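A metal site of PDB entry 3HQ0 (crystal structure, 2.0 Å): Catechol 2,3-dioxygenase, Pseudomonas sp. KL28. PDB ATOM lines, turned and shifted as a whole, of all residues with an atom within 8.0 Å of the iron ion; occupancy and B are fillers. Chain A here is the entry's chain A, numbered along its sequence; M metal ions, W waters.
The backbone carbonyl oxygen of His 154 lies within hydrogen-bond range of the backbone NH of Ser 218.
N of Leu 156 lies within hydrogen-bond range of O of His 216 (2.8 Å).
The side-chain carboxylate (OE2) of Glu 267 sits at hydrogen-bond distance from the side-chain hydroxyl (OG1) of Thr 255 (2.7 Å).
The side-chain carboxylate of Glu 267 sits close to the side-chain hydroxyl of Ser 218, 2.9 Å away.
A ring nitrogen (ND1) of His 154 sits at hydrogen-bond distance from the side-chain carboxylate (OD2) of Asp 153 (2.8 Å).
The backbone carbonyl oxygen of Ser 218 is in hydrogen-bond range of the backbone NH of Asp 153, at 2.8 Å.
NE2 of His 154 lies close to NE2 of His 201 (3.0 Å).
N of Glu 267 is in hydrogen-bond range of O of Cys 217 (2.8 Å).
Residues that only touch the iron ion: His 201 and Ser 218.
Within 4 Å of the iron ion: His 154, His 201, His 216, Ser 218 and Glu 267.
Along chain A the residues within 4 Å of the iron ion span positions 154 to 267.
The nearest printed residue that does not touch the iron ion is Tyr 257 (4.1 Å).
NE2 of His 154 is bound to the iron ion (2.2 Å).
OE1 of Glu 267 binds the iron ion (2.2 Å).
The iron ion is bound by NE2 of His 216, 2.4 Å away.
The iron ion has three donor atoms within binding distance.
Water W1 lies within hydrogen-bond range of the side-chain carboxylate of Asp 294 and the indole nitrogen of Trp 193.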
ATOM      1  N   ASP A 153      20.031  14.631  -3.795  1.00  0.00           N
ATOM      2  CA  ASP A 153      20.691  15.770  -4.405  1.00  0.00           C
ATOM      3  C   ASP A 153      22.133  15.540  -4.827  1.00  0.00           C
ATOM      4  O   ASP A 153      22.539  15.921  -5.922  1.00  0.00           O
ATOM      5  CB  ASP A 153      20.617  16.960  -3.443  1.00  0.00           C
ATOM      6  CG  ASP A 153      20.794  18.270  -4.140  1.00  0.00           C
ATOM      7  OD1 ASP A 153      19.801  18.765  -4.739  1.00  0.00           O
ATOM      8  OD2 ASP A 153      21.918  18.794  -4.121  1.00  0.00           O
ATOM      9  N   HIS A 154      22.925  14.941  -3.945  1.00  0.00           N
ATOM     10  CA  HIS A 154      24.330  14.669  -4.235  1.00  0.00           C
ATOM     11  C   HIS A 154      24.917  13.954  -3.034  1.00  0.00           C
ATOM     12  O   HIS A 154      24.194  13.525  -2.136  1.00  0.00           O
ATOM     13  CB  HIS A 154      25.102  15.983  -4.444  1.00  0.00           C
ATOM     14  CG  HIS A 154      25.191  16.842  -3.211  1.00  0.00           C
ATOM     15  ND1 HIS A 154      24.207  17.743  -2.869  1.00  0.00           N
ATOM     16  CD2 HIS A 154      26.077  16.857  -2.197  1.00  0.00           C
ATOM     17  CE1 HIS A 154      24.482  18.276  -1.690  1.00  0.00           C
ATOM     18  NE2 HIS A 154      25.615  17.746  -1.261  1.00  0.00           N
ATOM     19  N   CYS A 155      26.231  13.829  -3.035  1.00  0.00           N
ATOM     20  CA  CYS A 155      26.940  13.233  -1.916  1.00  0.00           C
ATOM     21  C   CYS A 155      28.296  13.935  -1.885  1.00  0.00           C
ATOM     22  O   CYS A 155      28.663  14.623  -2.834  1.00  0.00           O
ATOM     23  CB  CYS A 155      27.088  11.712  -2.083  1.00  0.00           C
ATOM     24  SG  CYS A 155      28.304  11.171  -3.299  1.00  0.00           S
ATOM     25  N   LEU A 156      29.010  13.800  -0.772  1.00  0.00           N
ATOM     26  CA  LEU A 156      30.323  14.411  -0.679  1.00  0.00           C
ATOM     27  C   LEU A 156      31.240  13.314  -0.194  1.00  0.00           C
ATOM     28  O   LEU A 156      31.064  12.784   0.900  1.00  0.00           O
ATOM     29  CB  LEU A 156      30.309  15.596   0.305  1.00  0.00           C
ATOM     30  CG  LEU A 156      31.636  16.366   0.394  1.00  0.00           C
ATOM     31  CD1 LEU A 156      31.393  17.769   0.906  1.00  0.00           C
ATOM     32  CD2 LEU A 156      32.591  15.630   1.302  1.00  0.00           C
ATOM     33  N   TRP A 193      33.477  20.901  -5.882  1.00  0.00           N
ATOM     34  CA  TRP A 193      32.043  20.717  -5.989  1.00  0.00           C
ATOM     35  C   TRP A 193      31.760  20.701  -7.479  1.00  0.00           C
ATOM     36  O   TRP A 193      31.923  21.704  -8.180  1.00  0.00           O
ATOM     37  CB  TRP A 193      31.332  21.864  -5.268  1.00  0.00           C
ATOM     38  CG  TRP A 193      31.345  21.661  -3.778  1.00  0.00           C
ATOM     39  CD1 TRP A 193      30.327  21.168  -3.011  1.00  0.00           C
ATOM     40  CD2 TRP A 193      32.452  21.853  -2.896  1.00  0.00           C
ATOM     41  NE1 TRP A 193      30.743  21.030  -1.712  1.00  0.00           N
ATOM     42  CE2 TRP A 193      32.047  21.445  -1.606  1.00  0.00           C
ATOM     43  CE3 TRP A 193      33.768  22.333  -3.070  1.00  0.00           C
ATOM     44  CZ2 TRP A 193      32.885  21.496  -0.492  1.00  0.00           C
ATOM     45  CZ3 TRP A 193      34.613  22.385  -1.963  1.00  0.00           C
ATOM     46  CH2 TRP A 193      34.162  21.967  -0.688  1.00  0.00           C
ATOM     47  N   HIS A 201      25.860  21.564  -7.310  1.00  0.00           N
ATOM     48  CA  HIS A 201      26.669  20.369  -7.416  1.00  0.00           C
ATOM     49  C   HIS A 201      25.885  19.067  -7.359  1.00  0.00           C
ATOM     50  O   HIS A 201      24.861  18.934  -6.672  1.00  0.00           O
ATOM     51  CB  HIS A 201      27.827  20.364  -6.390  1.00  0.00           C
ATOM     52  CG  HIS A 201      27.379  20.309  -4.961  1.00  0.00           C
ATOM     53  ND1 HIS A 201      26.567  21.269  -4.396  1.00  0.00           N
ATOM     54  CD2 HIS A 201      27.674  19.428  -3.965  1.00  0.00           C
ATOM     55  CE1 HIS A 201      26.388  20.992  -3.111  1.00  0.00           C
ATOM     56  NE2 HIS A 201      27.048  19.885  -2.831  1.00  0.00           N
ATOM     57  N   ALA A 204      30.553  15.989  -4.813  1.00  0.00           N
ATOM     58  CA  ALA A 204      31.684  16.757  -4.305  1.00  0.00           C
ATOM     59  C   ALA A 204      32.738  15.847  -3.674  1.00  0.00           C
ATOM     60  O   ALA A 204      32.426  14.745  -3.213  1.00  0.00           O
ATOM     61  CB  ALA A 204      31.200  17.787  -3.247  1.00  0.00           C
ATOM     62  N   HIS A 215      31.365  11.069   3.390  1.00  0.00           N
ATOM     63  CA  HIS A 215      31.085  12.114   4.358  1.00  0.00           C
ATOM     64  C   HIS A 215      29.569  12.121   4.532  1.00  0.00           C
ATOM     65  O   HIS A 215      29.067  11.942   5.634  1.00  0.00           O
ATOM     66  CB  HIS A 215      31.566  13.483   3.863  1.00  0.00           C
ATOM     67  CG  HIS A 215      31.382  14.576   4.869  1.00  0.00           C
ATOM     68  ND1 HIS A 215      32.183  14.711   5.973  1.00  0.00           N
ATOM     69  CD2 HIS A 215      30.471  15.574   4.936  1.00  0.00           C
ATOM     70  CE1 HIS A 215      31.777  15.755   6.687  1.00  0.00           C
ATOM     71  NE2 HIS A 215      30.743  16.291   6.077  1.00  0.00           N
ATOM     72  N   HIS A 216      28.850  12.337   3.434  1.00  0.00           N
ATOM     73  CA  HIS A 216      27.390  12.334   3.494  1.00  0.00           C
ATOM     74  C   HIS A 216      26.690  12.246   2.155  1.00  0.00           C
ATOM     75  O   HIS A 216      27.258  12.599   1.110  1.00  0.00           O
ATOM     76  CB  HIS A 216      26.853  13.586   4.214  1.00  0.00           C
ATOM     77  CG  HIS A 216      26.992  14.849   3.421  1.00  0.00           C
ATOM     78  ND1 HIS A 216      28.119  15.635   3.452  1.00  0.00           N
ATOM     79  CD2 HIS A 216      26.132  15.459   2.563  1.00  0.00           C
ATOM     80  CE1 HIS A 216      27.963  16.665   2.648  1.00  0.00           C
ATOM     81  NE2 HIS A 216      26.759  16.585   2.095  1.00  0.00           N
ATOM     82  N   CYS A 217      25.452  11.790   2.202  1.00  0.00           N
ATOM     83  CA  CYS A 217      24.578  11.742   1.031  1.00  0.00           C
ATOM     84  C   CYS A 217      23.620  12.899   1.335  1.00  0.00           C
ATOM     85  O   CYS A 217      23.315  13.140   2.503  1.00  0.00           O
ATOM     86  CB  CYS A 217      23.814  10.427   0.968  1.00  0.00           C
ATOM     87  SG  CYS A 217      24.771   9.117   0.216  1.00  0.00           S
ATOM     88  N   SER A 218      23.161  13.600   0.305  1.00  0.00           N
ATOM     89  CA  SER A 218      22.288  14.742   0.557  1.00  0.00           C
ATOM     90  C   SER A 218      20.905  14.678  -0.063  1.00  0.00           C
ATOM     91  O   SER A 218      20.722  14.183  -1.170  1.00  0.00           O
ATOM     92  CB  SER A 218      22.971  16.040   0.124  1.00  0.00           C
ATOM     93  OG  SER A 218      22.095  17.144   0.272  1.00  0.00           O
ATOM     94  N   PHE A 219      19.934  15.212   0.681  1.00  0.00           N
ATOM     95  CA  PHE A 219      18.534  15.257   0.245  1.00  0.00           C
ATOM     96  C   PHE A 219      17.974  16.670   0.240  1.00  0.00           C
ATOM     97  O   PHE A 219      18.069  17.403   1.223  1.00  0.00           O
ATOM     98  CB  PHE A 219      17.696  14.341   1.143  1.00  0.00           C
ATOM     99  CG  PHE A 219      18.101  12.898   1.077  1.00  0.00           C
ATOM    100  CD1 PHE A 219      19.162  12.431   1.845  1.00  0.00           C
ATOM    101  CD2 PHE A 219      17.469  12.023   0.193  1.00  0.00           C
ATOM    102  CE1 PHE A 219      19.593  11.097   1.733  1.00  0.00           C
ATOM    103  CE2 PHE A 219      17.884  10.695   0.070  1.00  0.00           C
ATOM    104  CZ  PHE A 219      18.954  10.234   0.847  1.00  0.00           C
ATOM    105  N   HIS A 248      25.136  27.523   5.049  1.00  0.00           N
ATOM    106  CA  HIS A 248      26.373  26.949   4.560  1.00  0.00           C
ATOM    107  C   HIS A 248      27.336  28.064   4.145  1.00  0.00           C
ATOM    108  O   HIS A 248      27.717  28.907   4.943  1.00  0.00           O
ATOM    109  CB  HIS A 248      26.097  26.041   3.357  1.00  0.00           C
ATOM    110  CG  HIS A 248      26.462  24.610   3.579  1.00  0.00           C
ATOM    111  ND1 HIS A 248      26.106  23.610   2.698  1.00  0.00           N
ATOM    112  CD2 HIS A 248      27.154  24.006   4.575  1.00  0.00           C
ATOM    113  CE1 HIS A 248      26.562  22.449   3.153  1.00  0.00           C
ATOM    114  NE2 HIS A 248      27.203  22.668   4.288  1.00  0.00           N
ATOM    115  N   VAL A 250      29.657  27.300   1.031  1.00  0.00           N
ATOM    116  CA  VAL A 250      30.155  26.627  -0.169  1.00  0.00           C
ATOM    117  C   VAL A 250      28.963  26.086  -0.967  1.00  0.00           C
ATOM    118  O   VAL A 250      29.005  24.957  -1.450  1.00  0.00           O
ATOM    119  CB  VAL A 250      31.106  25.466   0.184  1.00  0.00           C
ATOM    120  CG1 VAL A 250      32.300  25.980   0.964  1.00  0.00           C
ATOM    121  CG2 VAL A 250      30.371  24.407   0.989  1.00  0.00           C
ATOM    122  N   THR A 251      27.920  26.909  -1.078  1.00  0.00           N
ATOM    123  CA  THR A 251      26.708  26.516  -1.805  1.00  0.00           C
ATOM    124  C   THR A 251      25.545  27.450  -1.486  1.00  0.00           C
ATOM    125  O   THR A 251      24.496  27.377  -2.120  1.00  0.00           O
ATOM    126  CB  THR A 251      26.280  25.074  -1.456  1.00  0.00           C
ATOM    127  OG1 THR A 251      25.072  24.741  -2.138  1.00  0.00           O
ATOM    128  CG2 THR A 251      26.057  24.940   0.051  1.00  0.00           C
ATOM    129  N   THR A 255      21.174  24.211   5.677  1.00  0.00           N
ATOM    130  CA  THR A 255      21.109  22.776   5.894  1.00  0.00           C
ATOM    131  C   THR A 255      21.306  22.260   7.320  1.00  0.00           C
ATOM    132  O   THR A 255      21.644  23.006   8.230  1.00  0.00           O
ATOM    133  CB  THR A 255      22.186  22.144   4.992  1.00  0.00           C
ATOM    134  OG1 THR A 255      22.324  20.736   5.267  1.00  0.00           O
ATOM    135  CG2 THR A 255      23.514  22.849   5.238  1.00  0.00           C
ATOM    136  N   TYR A 257      23.087  18.647   9.132  1.00  0.00           N
ATOM    137  CA  TYR A 257      23.802  17.383   8.956  1.00  0.00           C
ATOM    138  C   TYR A 257      23.394  16.497  10.118  1.00  0.00           C
ATOM    139  O   TYR A 257      23.455  16.916  11.277  1.00  0.00           O
ATOM    140  CB  TYR A 257      25.324  17.565   9.032  1.00  0.00           C
ATOM    141  CG  TYR A 257      25.983  18.059   7.764  1.00  0.00           C
ATOM    142  CD1 TYR A 257      25.268  18.210   6.574  1.00  0.00           C
ATOM    143  CD2 TYR A 257      27.344  18.386   7.764  1.00  0.00           C
ATOM    144  CE1 TYR A 257      25.888  18.667   5.425  1.00  0.00           C
ATOM    145  CE2 TYR A 257      27.971  18.845   6.607  1.00  0.00           C
ATOM    146  CZ  TYR A 257      27.236  18.981   5.437  1.00  0.00           C
ATOM    147  OH  TYR A 257      27.845  19.458   4.296  1.00  0.00           O
ATOM    148  N   PHE A 266      23.865  12.096   6.701  1.00  0.00           N
ATOM    149  CA  PHE A 266      23.088  12.530   5.553  1.00  0.00           C
ATOM    150  C   PHE A 266      22.787  14.001   5.740  1.00  0.00           C
ATOM    151  O   PHE A 266      22.937  14.535   6.841  1.00  0.00           O
ATOM    152  CB  PHE A 266      21.790  11.721   5.439  1.00  0.00           C
ATOM    153  CG  PHE A 266      20.864  11.909   6.604  1.00  0.00           C
ATOM    154  CD1 PHE A 266      19.821  12.822   6.540  1.00  0.00           C
ATOM    155  CD2 PHE A 266      21.036  11.168   7.768  1.00  0.00           C
ATOM    156  CE1 PHE A 266      18.956  12.995   7.632  1.00  0.00           C
ATOM    157  CE2 PHE A 266      20.190  11.332   8.848  1.00  0.00           C
ATOM    158  CZ  PHE A 266      19.147  12.245   8.784  1.00  0.00           C
ATOM    159  N   GLU A 267      22.378  14.679   4.667  1.00  0.00           N
ATOM    160  CA  GLU A 267      22.050  16.098   4.739  1.00  0.00           C
ATOM    161  C   GLU A 267      20.653  16.390   4.205  1.00  0.00           C
ATOM    162  O   GLU A 267      20.219  15.776   3.230  1.00  0.00           O
ATOM    163  CB  GLU A 267      23.076  16.938   3.954  1.00  0.00           C
ATOM    164  CG  GLU A 267      22.586  18.354   3.611  1.00  0.00           C
ATOM    165  CD  GLU A 267      23.574  19.129   2.753  1.00  0.00           C
ATOM    166  OE1 GLU A 267      24.098  18.563   1.785  1.00  0.00           O
ATOM    167  OE2 GLU A 267      23.820  20.319   3.041  1.00  0.00           O
ATOM    168  N   THR A 268      19.964  17.325   4.854  1.00  0.00           N
ATOM    169  CA  THR A 268      18.633  17.748   4.407  1.00  0.00           C
ATOM    170  C   THR A 268      18.796  19.267   4.278  1.00  0.00           C
ATOM    171  O   THR A 268      18.955  19.949   5.289  1.00  0.00           O
ATOM    172  CB  THR A 268      17.523  17.430   5.443  1.00  0.00           C
ATOM    173  OG1 THR A 268      17.790  18.129   6.668  1.00  0.00           O
ATOM    174  CG2 THR A 268      17.444  15.940   5.702  1.00  0.00           C
ATOM    175  N   PHE A 269      18.774  19.775   3.052  1.00  0.00           N
ATOM    176  CA  PHE A 269      18.951  21.199   2.820  1.00  0.00           C
ATOM    177  C   PHE A 269      18.055  21.750   1.718  1.00  0.00           C
ATOM    178  O   PHE A 269      17.252  21.035   1.114  1.00  0.00           O
ATOM    179  CB  PHE A 269      20.389  21.483   2.396  1.00  0.00           C
ATOM    180  CG  PHE A 269      20.646  21.224   0.932  1.00  0.00           C
ATOM    181  CD1 PHE A 269      20.612  19.922   0.423  1.00  0.00           C
ATOM    182  CD2 PHE A 269      20.862  22.284   0.049  1.00  0.00           C
ATOM    183  CE1 PHE A 269      20.783  19.685  -0.949  1.00  0.00           C
ATOM    184  CE2 PHE A 269      21.034  22.056  -1.320  1.00  0.00           C
ATOM    185  CZ  PHE A 269      20.987  20.751  -1.813  1.00  0.00           C
ATOM    186  N   ASP A 294      32.292  20.982   6.083  1.00  0.00           N
ATOM    187  CA  ASP A 294      32.910  19.852   5.407  1.00  0.00           C
ATOM    188  C   ASP A 294      34.380  19.631   5.741  1.00  0.00           C
ATOM    189  O   ASP A 294      35.030  18.778   5.117  1.00  0.00           O
ATOM    190  CB  ASP A 294      32.744  19.979   3.890  1.00  0.00           C
ATOM    191  CG  ASP A 294      31.280  20.082   3.467  1.00  0.00           C
ATOM    192  OD1 ASP A 294      30.446  19.363   4.043  1.00  0.00           O
ATOM    193  OD2 ASP A 294      30.965  20.863   2.550  1.00  0.00           O
HETATM  194 FE    FE M   1      26.028  18.462   0.742  1.00  0.00          FE
HETATM  195  O   HOH W   1      28.927  20.388   0.553  1.00  0.00           O
HETATM  196  O   HOH W   2      24.882  21.228   0.033  1.00  0.00           O
